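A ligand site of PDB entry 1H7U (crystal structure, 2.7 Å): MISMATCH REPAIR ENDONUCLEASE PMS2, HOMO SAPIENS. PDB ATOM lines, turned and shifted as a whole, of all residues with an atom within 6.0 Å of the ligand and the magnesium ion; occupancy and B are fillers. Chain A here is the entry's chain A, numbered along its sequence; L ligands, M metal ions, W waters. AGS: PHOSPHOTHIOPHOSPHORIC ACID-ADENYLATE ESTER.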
ATOM      1  N   VAL A  31      -0.077   5.182  -8.808  1.00  0.00           N
ATOM      2  CA  VAL A  31      -0.603   5.899  -7.597  1.00  0.00           C
ATOM      3  C   VAL A  31       0.452   6.125  -6.480  1.00  0.00           C
ATOM      4  O   VAL A  31       0.459   5.463  -5.443  1.00  0.00           O
ATOM      5  CB  VAL A  31      -1.833   5.175  -6.999  1.00  0.00           C
ATOM      6  CG1 VAL A  31      -2.989   5.253  -7.975  1.00  0.00           C
ATOM      7  CG2 VAL A  31      -1.497   3.737  -6.680  1.00  0.00           C
ATOM      8  N   GLU A  41      -0.307   2.676   0.222  1.00  0.00           N
ATOM      9  CA  GLU A  41       0.002   1.608  -0.722  1.00  0.00           C
ATOM     10  C   GLU A  41       0.898   0.551  -0.087  1.00  0.00           C
ATOM     11  O   GLU A  41       0.682  -0.652  -0.233  1.00  0.00           O
ATOM     12  CB  GLU A  41       0.667   2.206  -1.950  1.00  0.00           C
ATOM     13  CG  GLU A  41      -0.305   2.883  -2.885  1.00  0.00           C
ATOM     14  CD  GLU A  41      -1.078   1.867  -3.680  1.00  0.00           C
ATOM     15  OE1 GLU A  41      -0.498   0.799  -3.965  1.00  0.00           O
ATOM     16  OE2 GLU A  41      -2.246   2.120  -4.022  1.00  0.00           O
ATOM     17  N   LEU A  42       1.911   1.029   0.635  1.00  0.00           N
ATOM     18  CA  LEU A  42       2.862   0.174   1.327  1.00  0.00           C
ATOM     19  C   LEU A  42       2.199  -0.588   2.465  1.00  0.00           C
ATOM     20  O   LEU A  42       2.408  -1.793   2.636  1.00  0.00           O
ATOM     21  CB  LEU A  42       3.979   1.047   1.871  1.00  0.00           C
ATOM     22  CG  LEU A  42       5.412   0.733   1.482  1.00  0.00           C
ATOM     23  CD1 LEU A  42       5.488   0.314   0.040  1.00  0.00           C
ATOM     24  CD2 LEU A  42       6.236   1.978   1.749  1.00  0.00           C
ATOM     25  N   GLU A  44      -0.929  -1.250   2.777  1.00  0.00           N
ATOM     26  CA  GLU A  44      -1.864  -2.210   2.246  1.00  0.00           C
ATOM     27  C   GLU A  44      -1.121  -3.447   1.773  1.00  0.00           C
ATOM     28  O   GLU A  44      -1.616  -4.569   1.933  1.00  0.00           O
ATOM     29  CB  GLU A  44      -2.696  -1.580   1.127  1.00  0.00           C
ATOM     30  CG  GLU A  44      -4.081  -1.258   1.604  1.00  0.00           C
ATOM     31  CD  GLU A  44      -4.821  -0.397   0.634  1.00  0.00           C
ATOM     32  OE1 GLU A  44      -4.172   0.066  -0.334  1.00  0.00           O
ATOM     33  OE2 GLU A  44      -6.035  -0.166   0.838  1.00  0.00           O
ATOM     34  N   ASN A  45       0.075  -3.253   1.217  1.00  0.00           N
ATOM     35  CA  ASN A  45       0.860  -4.399   0.776  1.00  0.00           C
ATOM     36  C   ASN A  45       1.149  -5.313   1.957  1.00  0.00           C
ATOM     37  O   ASN A  45       1.057  -6.539   1.848  1.00  0.00           O
ATOM     38  CB  ASN A  45       2.179  -3.966   0.165  1.00  0.00           C
ATOM     39  CG  ASN A  45       2.082  -3.730  -1.307  1.00  0.00           C
ATOM     40  OD1 ASN A  45       1.180  -4.259  -1.981  1.00  0.00           O
ATOM     41  ND2 ASN A  45       3.000  -2.957  -1.851  1.00  0.00           N
ATOM     42  N   SER A  46       1.487  -4.719   3.092  1.00  0.00           N
ATOM     43  CA  SER A  46       1.766  -5.496   4.275  1.00  0.00           C
ATOM     44  C   SER A  46       0.532  -6.242   4.755  1.00  0.00           C
ATOM     45  O   SER A  46       0.615  -7.430   5.085  1.00  0.00           O
ATOM     46  CB  SER A  46       2.314  -4.584   5.371  1.00  0.00           C
ATOM     47  OG  SER A  46       3.548  -4.045   4.938  1.00  0.00           O
ATOM     48  N   ASP A  48      -2.101  -7.200   3.039  1.00  0.00           N
ATOM     49  CA  ASP A  48      -2.384  -8.250   2.071  1.00  0.00           C
ATOM     50  C   ASP A  48      -1.421  -9.416   2.222  1.00  0.00           C
ATOM     51  O   ASP A  48      -1.739 -10.542   1.836  1.00  0.00           O
ATOM     52  CB  ASP A  48      -2.295  -7.725   0.638  1.00  0.00           C
ATOM     53  CG  ASP A  48      -3.432  -6.817   0.284  1.00  0.00           C
ATOM     54  OD1 ASP A  48      -4.470  -6.847   0.974  1.00  0.00           O
ATOM     55  OD2 ASP A  48      -3.291  -6.065  -0.700  1.00  0.00           O
ATOM     56  N   ALA A  49      -0.248  -9.132   2.745  1.00  0.00           N
ATOM     57  CA  ALA A  49       0.771 -10.154   2.926  1.00  0.00           C
ATOM     58  C   ALA A  49       0.496 -10.939   4.221  1.00  0.00           C
ATOM     59  O   ALA A  49       1.255 -11.862   4.574  1.00  0.00           O
ATOM     60  CB  ALA A  49       2.144  -9.517   2.961  1.00  0.00           C
ATOM     61  N   ASP A  70       7.442  -5.452   7.835  1.00  0.00           N
ATOM     62  CA  ASP A  70       6.359  -6.342   8.260  1.00  0.00           C
ATOM     63  C   ASP A  70       6.748  -7.812   8.392  1.00  0.00           C
ATOM     64  O   ASP A  70       7.755  -8.258   7.823  1.00  0.00           O
ATOM     65  CB  ASP A  70       5.180  -6.247   7.283  1.00  0.00           C
ATOM     66  CG  ASP A  70       5.479  -6.895   5.937  1.00  0.00           C
ATOM     67  OD1 ASP A  70       5.769  -8.108   5.893  1.00  0.00           O
ATOM     68  OD2 ASP A  70       5.417  -6.176   4.903  1.00  0.00           O
ATOM     69  N   GLY A  72       4.771 -10.300   7.348  1.00  0.00           N
ATOM     70  CA  GLY A  72       3.835 -11.021   6.506  1.00  0.00           C
ATOM     71  C   GLY A  72       4.496 -12.231   5.864  1.00  0.00           C
ATOM     72  O   GLY A  72       5.498 -12.728   6.380  1.00  0.00           O
ATOM     73  N   CYS A  73       3.968 -12.679   4.722  1.00  0.00           N
ATOM     74  CA  CYS A  73       4.476 -13.872   4.025  1.00  0.00           C
ATOM     75  C   CYS A  73       5.776 -13.715   3.265  1.00  0.00           C
ATOM     76  O   CYS A  73       6.412 -14.714   2.907  1.00  0.00           O
ATOM     77  CB  CYS A  73       3.441 -14.380   3.043  1.00  0.00           C
ATOM     78  SG  CYS A  73       3.291 -13.307   1.617  1.00  0.00           S
ATOM     79  N   GLY A  74       6.180 -12.485   2.980  1.00  0.00           N
ATOM     80  CA  GLY A  74       7.420 -12.298   2.257  1.00  0.00           C
ATOM     81  C   GLY A  74       7.333 -12.687   0.788  1.00  0.00           C
ATOM     82  O   GLY A  74       6.257 -13.006   0.276  1.00  0.00           O
ATOM     83  N   VAL A  75       8.476 -12.682   0.122  1.00  0.00           N
ATOM     84  CA  VAL A  75       8.525 -12.996  -1.291  1.00  0.00           C
ATOM     85  C   VAL A  75       9.412 -14.168  -1.664  1.00  0.00           C
ATOM     86  O   VAL A  75      10.505 -14.371  -1.123  1.00  0.00           O
ATOM     87  CB  VAL A  75       8.986 -11.798  -2.099  1.00  0.00           C
ATOM     88  CG1 VAL A  75       8.909 -12.092  -3.576  1.00  0.00           C
ATOM     89  CG2 VAL A  75       8.125 -10.615  -1.758  1.00  0.00           C
ATOM     90  N   GLY A  82       9.529  -9.981 -10.761  1.00  0.00           N
ATOM     91  CA  GLY A  82       8.173  -9.551 -11.029  1.00  0.00           C
ATOM     92  C   GLY A  82       7.579  -8.607 -10.020  1.00  0.00           C
ATOM     93  O   GLY A  82       6.389  -8.311 -10.072  1.00  0.00           O
ATOM     94  N   LEU A  83       8.400  -8.136  -9.079  1.00  0.00           N
ATOM     95  CA  LEU A  83       7.928  -7.218  -8.047  1.00  0.00           C
ATOM     96  C   LEU A  83       7.585  -5.845  -8.628  1.00  0.00           C
ATOM     97  O   LEU A  83       6.565  -5.264  -8.251  1.00  0.00           O
ATOM     98  CB  LEU A  83       8.966  -7.071  -6.938  1.00  0.00           C
ATOM     99  CG  LEU A  83       8.996  -8.153  -5.859  1.00  0.00           C
ATOM    100  CD1 LEU A  83      10.195  -7.969  -4.941  1.00  0.00           C
ATOM    101  CD2 LEU A  83       7.710  -8.082  -5.064  1.00  0.00           C
ATOM    102  N   LEU A  85       6.487  -4.643 -11.746  1.00  0.00           N
ATOM    103  CA  LEU A  85       5.844  -4.991 -13.009  1.00  0.00           C
ATOM    104  C   LEU A  85       4.398  -5.618 -12.794  1.00  0.00           C
ATOM    105  O   LEU A  85       4.016  -5.865 -11.653  1.00  0.00           O
ATOM    106  CB  LEU A  85       6.776  -5.990 -13.664  1.00  0.00           C
ATOM    107  CG  LEU A  85       6.793  -6.118 -15.161  1.00  0.00           C
ATOM    108  CD1 LEU A  85       7.228  -4.793 -15.779  1.00  0.00           C
ATOM    109  CD2 LEU A  85       7.746  -7.218 -15.559  1.00  0.00           C
ATOM    110  N   LYS A  86       3.619  -5.833 -13.879  1.00  0.00           N
ATOM    111  CA  LYS A  86       2.246  -6.495 -13.968  1.00  0.00           C
ATOM    112  C   LYS A  86       0.889  -5.917 -13.512  1.00  0.00           C
ATOM    113  O   LYS A  86      -0.156  -6.621 -13.679  1.00  0.00           O
ATOM    114  CB  LYS A  86       2.316  -7.908 -13.365  1.00  0.00           C
ATOM    115  CG  LYS A  86       2.094  -7.941 -11.861  1.00  0.00           C
ATOM    116  CD  LYS A  86       2.800  -9.117 -11.213  1.00  0.00           C
ATOM    117  CE  LYS A  86       2.927  -8.906  -9.706  1.00  0.00           C
ATOM    118  NZ  LYS A  86       3.477  -7.561  -9.367  1.00  0.00           N
ATOM    119  N   GLY A 108      -3.535   0.360  -9.441  1.00  0.00           N
ATOM    120  CA  GLY A 108      -2.794  -0.668 -10.140  1.00  0.00           C
ATOM    121  C   GLY A 108      -1.288  -0.496 -10.346  1.00  0.00           C
ATOM    122  O   GLY A 108      -0.853   0.407 -11.070  1.00  0.00           O
ATOM    123  N   GLU A 109      -0.552  -1.401  -9.699  1.00  0.00           N
ATOM    124  CA  GLU A 109       0.891  -1.556  -9.690  1.00  0.00           C
ATOM    125  C   GLU A 109       1.801  -0.318  -9.502  1.00  0.00           C
ATOM    126  O   GLU A 109       2.470   0.208 -10.402  1.00  0.00           O
ATOM    127  CB  GLU A 109       1.235  -2.438 -10.889  1.00  0.00           C
ATOM    128  CG  GLU A 109       0.183  -3.590 -11.014  1.00  0.00           C
ATOM    129  CD  GLU A 109       0.553  -4.896 -10.274  1.00  0.00           C
ATOM    130  OE1 GLU A 109       1.733  -5.074  -9.894  1.00  0.00           O
ATOM    131  OE2 GLU A 109      -0.346  -5.766 -10.098  1.00  0.00           O
ATOM    132  N   ALA A 110       1.819   0.053  -8.233  1.00  0.00           N
ATOM    133  CA  ALA A 110       2.522   1.177  -7.664  1.00  0.00           C
ATOM    134  C   ALA A 110       3.878   0.820  -7.070  1.00  0.00           C
ATOM    135  O   ALA A 110       4.623   1.693  -6.609  1.00  0.00           O
ATOM    136  CB  ALA A 110       1.644   1.802  -6.595  1.00  0.00           C
ATOM    137  N   LEU A 111       4.240  -0.447  -7.046  1.00  0.00           N
ATOM    138  CA  LEU A 111       5.552  -0.784  -6.517  1.00  0.00           C
ATOM    139  C   LEU A 111       6.576  -0.359  -7.561  1.00  0.00           C
ATOM    140  O   LEU A 111       7.674   0.095  -7.230  1.00  0.00           O
ATOM    141  CB  LEU A 111       5.681  -2.272  -6.223  1.00  0.00           C
ATOM    142  CG  LEU A 111       6.090  -2.591  -4.779  1.00  0.00           C
ATOM    143  CD1 LEU A 111       6.714  -3.968  -4.681  1.00  0.00           C
ATOM    144  CD2 LEU A 111       7.089  -1.560  -4.285  1.00  0.00           C
ATOM    145  N   SER A 112       6.209  -0.512  -8.834  1.00  0.00           N
ATOM    146  CA  SER A 112       7.076  -0.131  -9.930  1.00  0.00           C
ATOM    147  C   SER A 112       7.213   1.378  -9.955  1.00  0.00           C
ATOM    148  O   SER A 112       8.274   1.921 -10.224  1.00  0.00           O
ATOM    149  CB  SER A 112       6.503  -0.611 -11.257  1.00  0.00           C
ATOM    150  OG  SER A 112       5.129  -0.278 -11.329  1.00  0.00           O
ATOM    151  N   THR A 124      13.598  -9.440   1.901  1.00  0.00           N
ATOM    152  CA  THR A 124      12.447 -10.300   2.105  1.00  0.00           C
ATOM    153  C   THR A 124      12.825 -11.758   2.308  1.00  0.00           C
ATOM    154  O   THR A 124      13.905 -12.171   1.914  1.00  0.00           O
ATOM    155  CB  THR A 124      11.470 -10.219   0.904  1.00  0.00           C
ATOM    156  OG1 THR A 124      10.250 -10.897   1.222  1.00  0.00           O
ATOM    157  CG2 THR A 124      12.086 -10.833  -0.338  1.00  0.00           C
ATOM    158  N   GLY A 154       9.024 -12.251   6.170  1.00  0.00           N
ATOM    159  CA  GLY A 154       8.420 -10.942   6.068  1.00  0.00           C
ATOM    160  C   GLY A 154       9.102 -10.116   4.997  1.00  0.00           C
ATOM    161  O   GLY A 154       9.933 -10.638   4.225  1.00  0.00           O
ATOM    162  N   THR A 155       8.779  -8.834   4.946  1.00  0.00           N
ATOM    163  CA  THR A 155       9.375  -7.979   3.936  1.00  0.00           C
ATOM    164  C   THR A 155       9.632  -6.621   4.520  1.00  0.00           C
ATOM    165  O   THR A 155       8.899  -6.177   5.397  1.00  0.00           O
ATOM    166  CB  THR A 155       8.434  -7.782   2.743  1.00  0.00           C
ATOM    167  OG1 THR A 155       8.035  -9.066   2.230  1.00  0.00           O
ATOM    168  CG2 THR A 155       9.115  -6.972   1.653  1.00  0.00           C
ATOM    169  N   VAL A 157      10.372  -2.796   3.019  1.00  0.00           N
ATOM    170  CA  VAL A 157      10.504  -1.923   1.858  1.00  0.00           C
ATOM    171  C   VAL A 157      11.015  -0.557   2.269  1.00  0.00           C
ATOM    172  O   VAL A 157      10.430   0.091   3.137  1.00  0.00           O
ATOM    173  CB  VAL A 157       9.149  -1.756   1.165  1.00  0.00           C
ATOM    174  CG1 VAL A 157       9.313  -0.952  -0.138  1.00  0.00           C
ATOM    175  CG2 VAL A 157       8.571  -3.111   0.859  1.00  0.00           C
HETATM  176  PG  AGS L   1      -2.761  -2.834  -5.947  1.00  0.00           P
HETATM  177  S1G AGS L   1      -4.317  -3.185  -4.927  1.00  0.00           S
HETATM  178  O2G AGS L   1      -2.951  -2.932  -7.281  1.00  0.00           O
HETATM  179  O3G AGS L   1      -2.064  -1.669  -5.327  1.00  0.00           O
HETATM  180  PB  AGS L   1      -1.088  -5.231  -5.722  1.00  0.00           P
HETATM  181  O1B AGS L   1      -0.520  -5.845  -4.590  1.00  0.00           O
HETATM  182  O2B AGS L   1      -1.333  -6.154  -7.030  1.00  0.00           O
HETATM  183  O3B AGS L   1      -1.639  -3.958  -5.343  1.00  0.00           O
HETATM  184  PA  AGS L   1       1.496  -3.793  -6.067  1.00  0.00           P
HETATM  185  O1A AGS L   1       1.497  -2.830  -5.090  1.00  0.00           O
HETATM  186  O2A AGS L   1       2.625  -3.501  -7.164  1.00  0.00           O
HETATM  187  O3A AGS L   1       0.497  -4.924  -5.740  1.00  0.00           O
HETATM  188  O5' AGS L   1       2.215  -4.851  -5.532  1.00  0.00           O
HETATM  189  C5' AGS L   1       2.764  -6.016  -5.497  1.00  0.00           C
HETATM  190  C4' AGS L   1       3.573  -7.277  -5.620  1.00  0.00           C
HETATM  191  O4' AGS L   1       4.731  -7.066  -4.725  1.00  0.00           O
HETATM  192  C3' AGS L   1       2.502  -8.049  -5.027  1.00  0.00           C
HETATM  193  O3' AGS L   1       1.647  -8.803  -5.857  1.00  0.00           O
HETATM  194  C2' AGS L   1       3.202  -8.828  -3.888  1.00  0.00           C
HETATM  195  O2' AGS L   1       3.406 -10.181  -4.283  1.00  0.00           O
HETATM  196  C1' AGS L   1       4.558  -8.074  -3.619  1.00  0.00           C
HETATM  197  N9  AGS L   1       4.619  -7.345  -2.323  1.00  0.00           N
HETATM  198  C8  AGS L   1       4.599  -5.968  -2.048  1.00  0.00           C
HETATM  199  N7  AGS L   1       4.682  -5.664  -0.795  1.00  0.00           N
HETATM  200  C5  AGS L   1       4.759  -6.916  -0.197  1.00  0.00           C
HETATM  201  C6  AGS L   1       4.862  -7.345   1.183  1.00  0.00           C
HETATM  202  N6  AGS L   1       4.919  -6.482   2.192  1.00  0.00           N
HETATM  203  N1  AGS L   1       4.932  -8.714   1.456  1.00  0.00           N
HETATM  204  C2  AGS L   1       4.879  -9.617   0.452  1.00  0.00           C
HETATM  205  N3  AGS L   1       4.773  -9.340  -0.868  1.00  0.00           N
HETATM  206  C4  AGS L   1       4.724  -7.942  -1.118  1.00  0.00           C
HETATM  207 MG    MG M   1      -0.357  -2.674  -3.527  1.00  0.00          MG
HETATM  208  O   HOH W   1       6.100  -9.801   3.839  1.00  0.00           O
HETATM  209  O   HOH W   2       5.335  -2.784  -0.483  1.00  0.00           O
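Water W1 lies within hydrogen-bond range of OG1 of Thr 155, OD1 of Asp 70, N of Gly 74 and N1 of the ligand.
Water W2 lies within hydrogen-bond range of ND2 of Asn 45 (2.7 Å) and N7 of the ligand (3.0 Å).
N of Leu 111 lies close to O2A of the ligand, at 3.5 Å.
ND2 of Asn 45 lies close to N7 of the ligand (3.4 Å).
O3G of the ligand sits at hydrogen-bond distance from OE1 of Glu 41, at 3.2 Å.
The side-chain carboxylate (OD2) of Asp 70 lies within hydrogen-bond range of a nitrogen (N6) of the ligand (2.8 Å).
The side-chain hydroxyl (OG1) of Thr 155 is in hydrogen-bond range of a nitrogen (N1) of the ligand, 3.2 Å away.
An oxygen (O2B) of the ligand sits close to the side-chain carboxylate of Glu 109 (3.2 Å).
Merely in contact with the ligand: Leu 83 (3.2 Å), Ala 49 (3.3 Å), Gly 108 (3.7 Å), Gly 74 (3.7 Å), Val 75 (3.7 Å), Lys 86 (3.8 Å), Ala 110 (3.8 Å) and Ser 46 (3.9 Å).
Within 4 Å of the ligand: Glu 41, Asn 45, Ser 46, Ala 49, Asp 70, Gly 74, Val 75, Leu 83, Lys 86, Gly 108, Glu 109, Ala 110, Leu 111 and Thr 155.
Residues that only touch the magnesium ion: Glu 41 (3.5 Å).
Two residues have an atom within 4 Å of the magnesium ion: Glu 41 and Asn 45.
The nearest printed residue that does not touch the magnesium ion is Asp 48 (5.3 Å).
The side-chain carboxylate (OD1) of Asp 70 sits at hydrogen-bond distance from the backbone NH (N) of Gly 72, at 2.8 Å.
O of Leu 42 sits at hydrogen-bond distance from OG of Ser 46, 3.4 Å away.
The side-chain carboxylate (OD2) of Asp 70 sits at hydrogen-bond distance from the side-chain hydroxyl (OG) of Ser 46 (2.8 Å).
The backbone carbonyl oxygen (O) of Glu 109 sits at hydrogen-bond distance from the side-chain hydroxyl (OG) of Ser 112 (2.9 Å).
The side-chain hydroxyl (OG1) of Thr 155 sits at hydrogen-bond distance from the side-chain hydroxyl (OG1) of Thr 124.
The backbone carbonyl oxygen (O) of Gly 82 lies within hydrogen-bond range of the side-chain amino group (NZ) of Lys 86.
N of Val 75 is in hydrogen-bond range of OG1 of Thr 124, at 2.7 Å.
The backbone NH (N) of Asp 70 lies within hydrogen-bond range of the backbone carbonyl oxygen (O) of Thr 155, 2.9 Å away.
O1A of the ligand is bound to the magnesium ion, 2.4 Å away.
An oxygen (O3B) of the ligand is bound to the magnesium ion, 2.6 Å away.
The magnesium ion has two donor atoms within binding distance.
Slightly farther from the magnesium ion lies an oxygen (O3G) of the ligand (2.7 Å).
Slightly farther from the magnesium ion lies the side-chain amide oxygen (OD1) of Asn 45 (2.7 Å).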
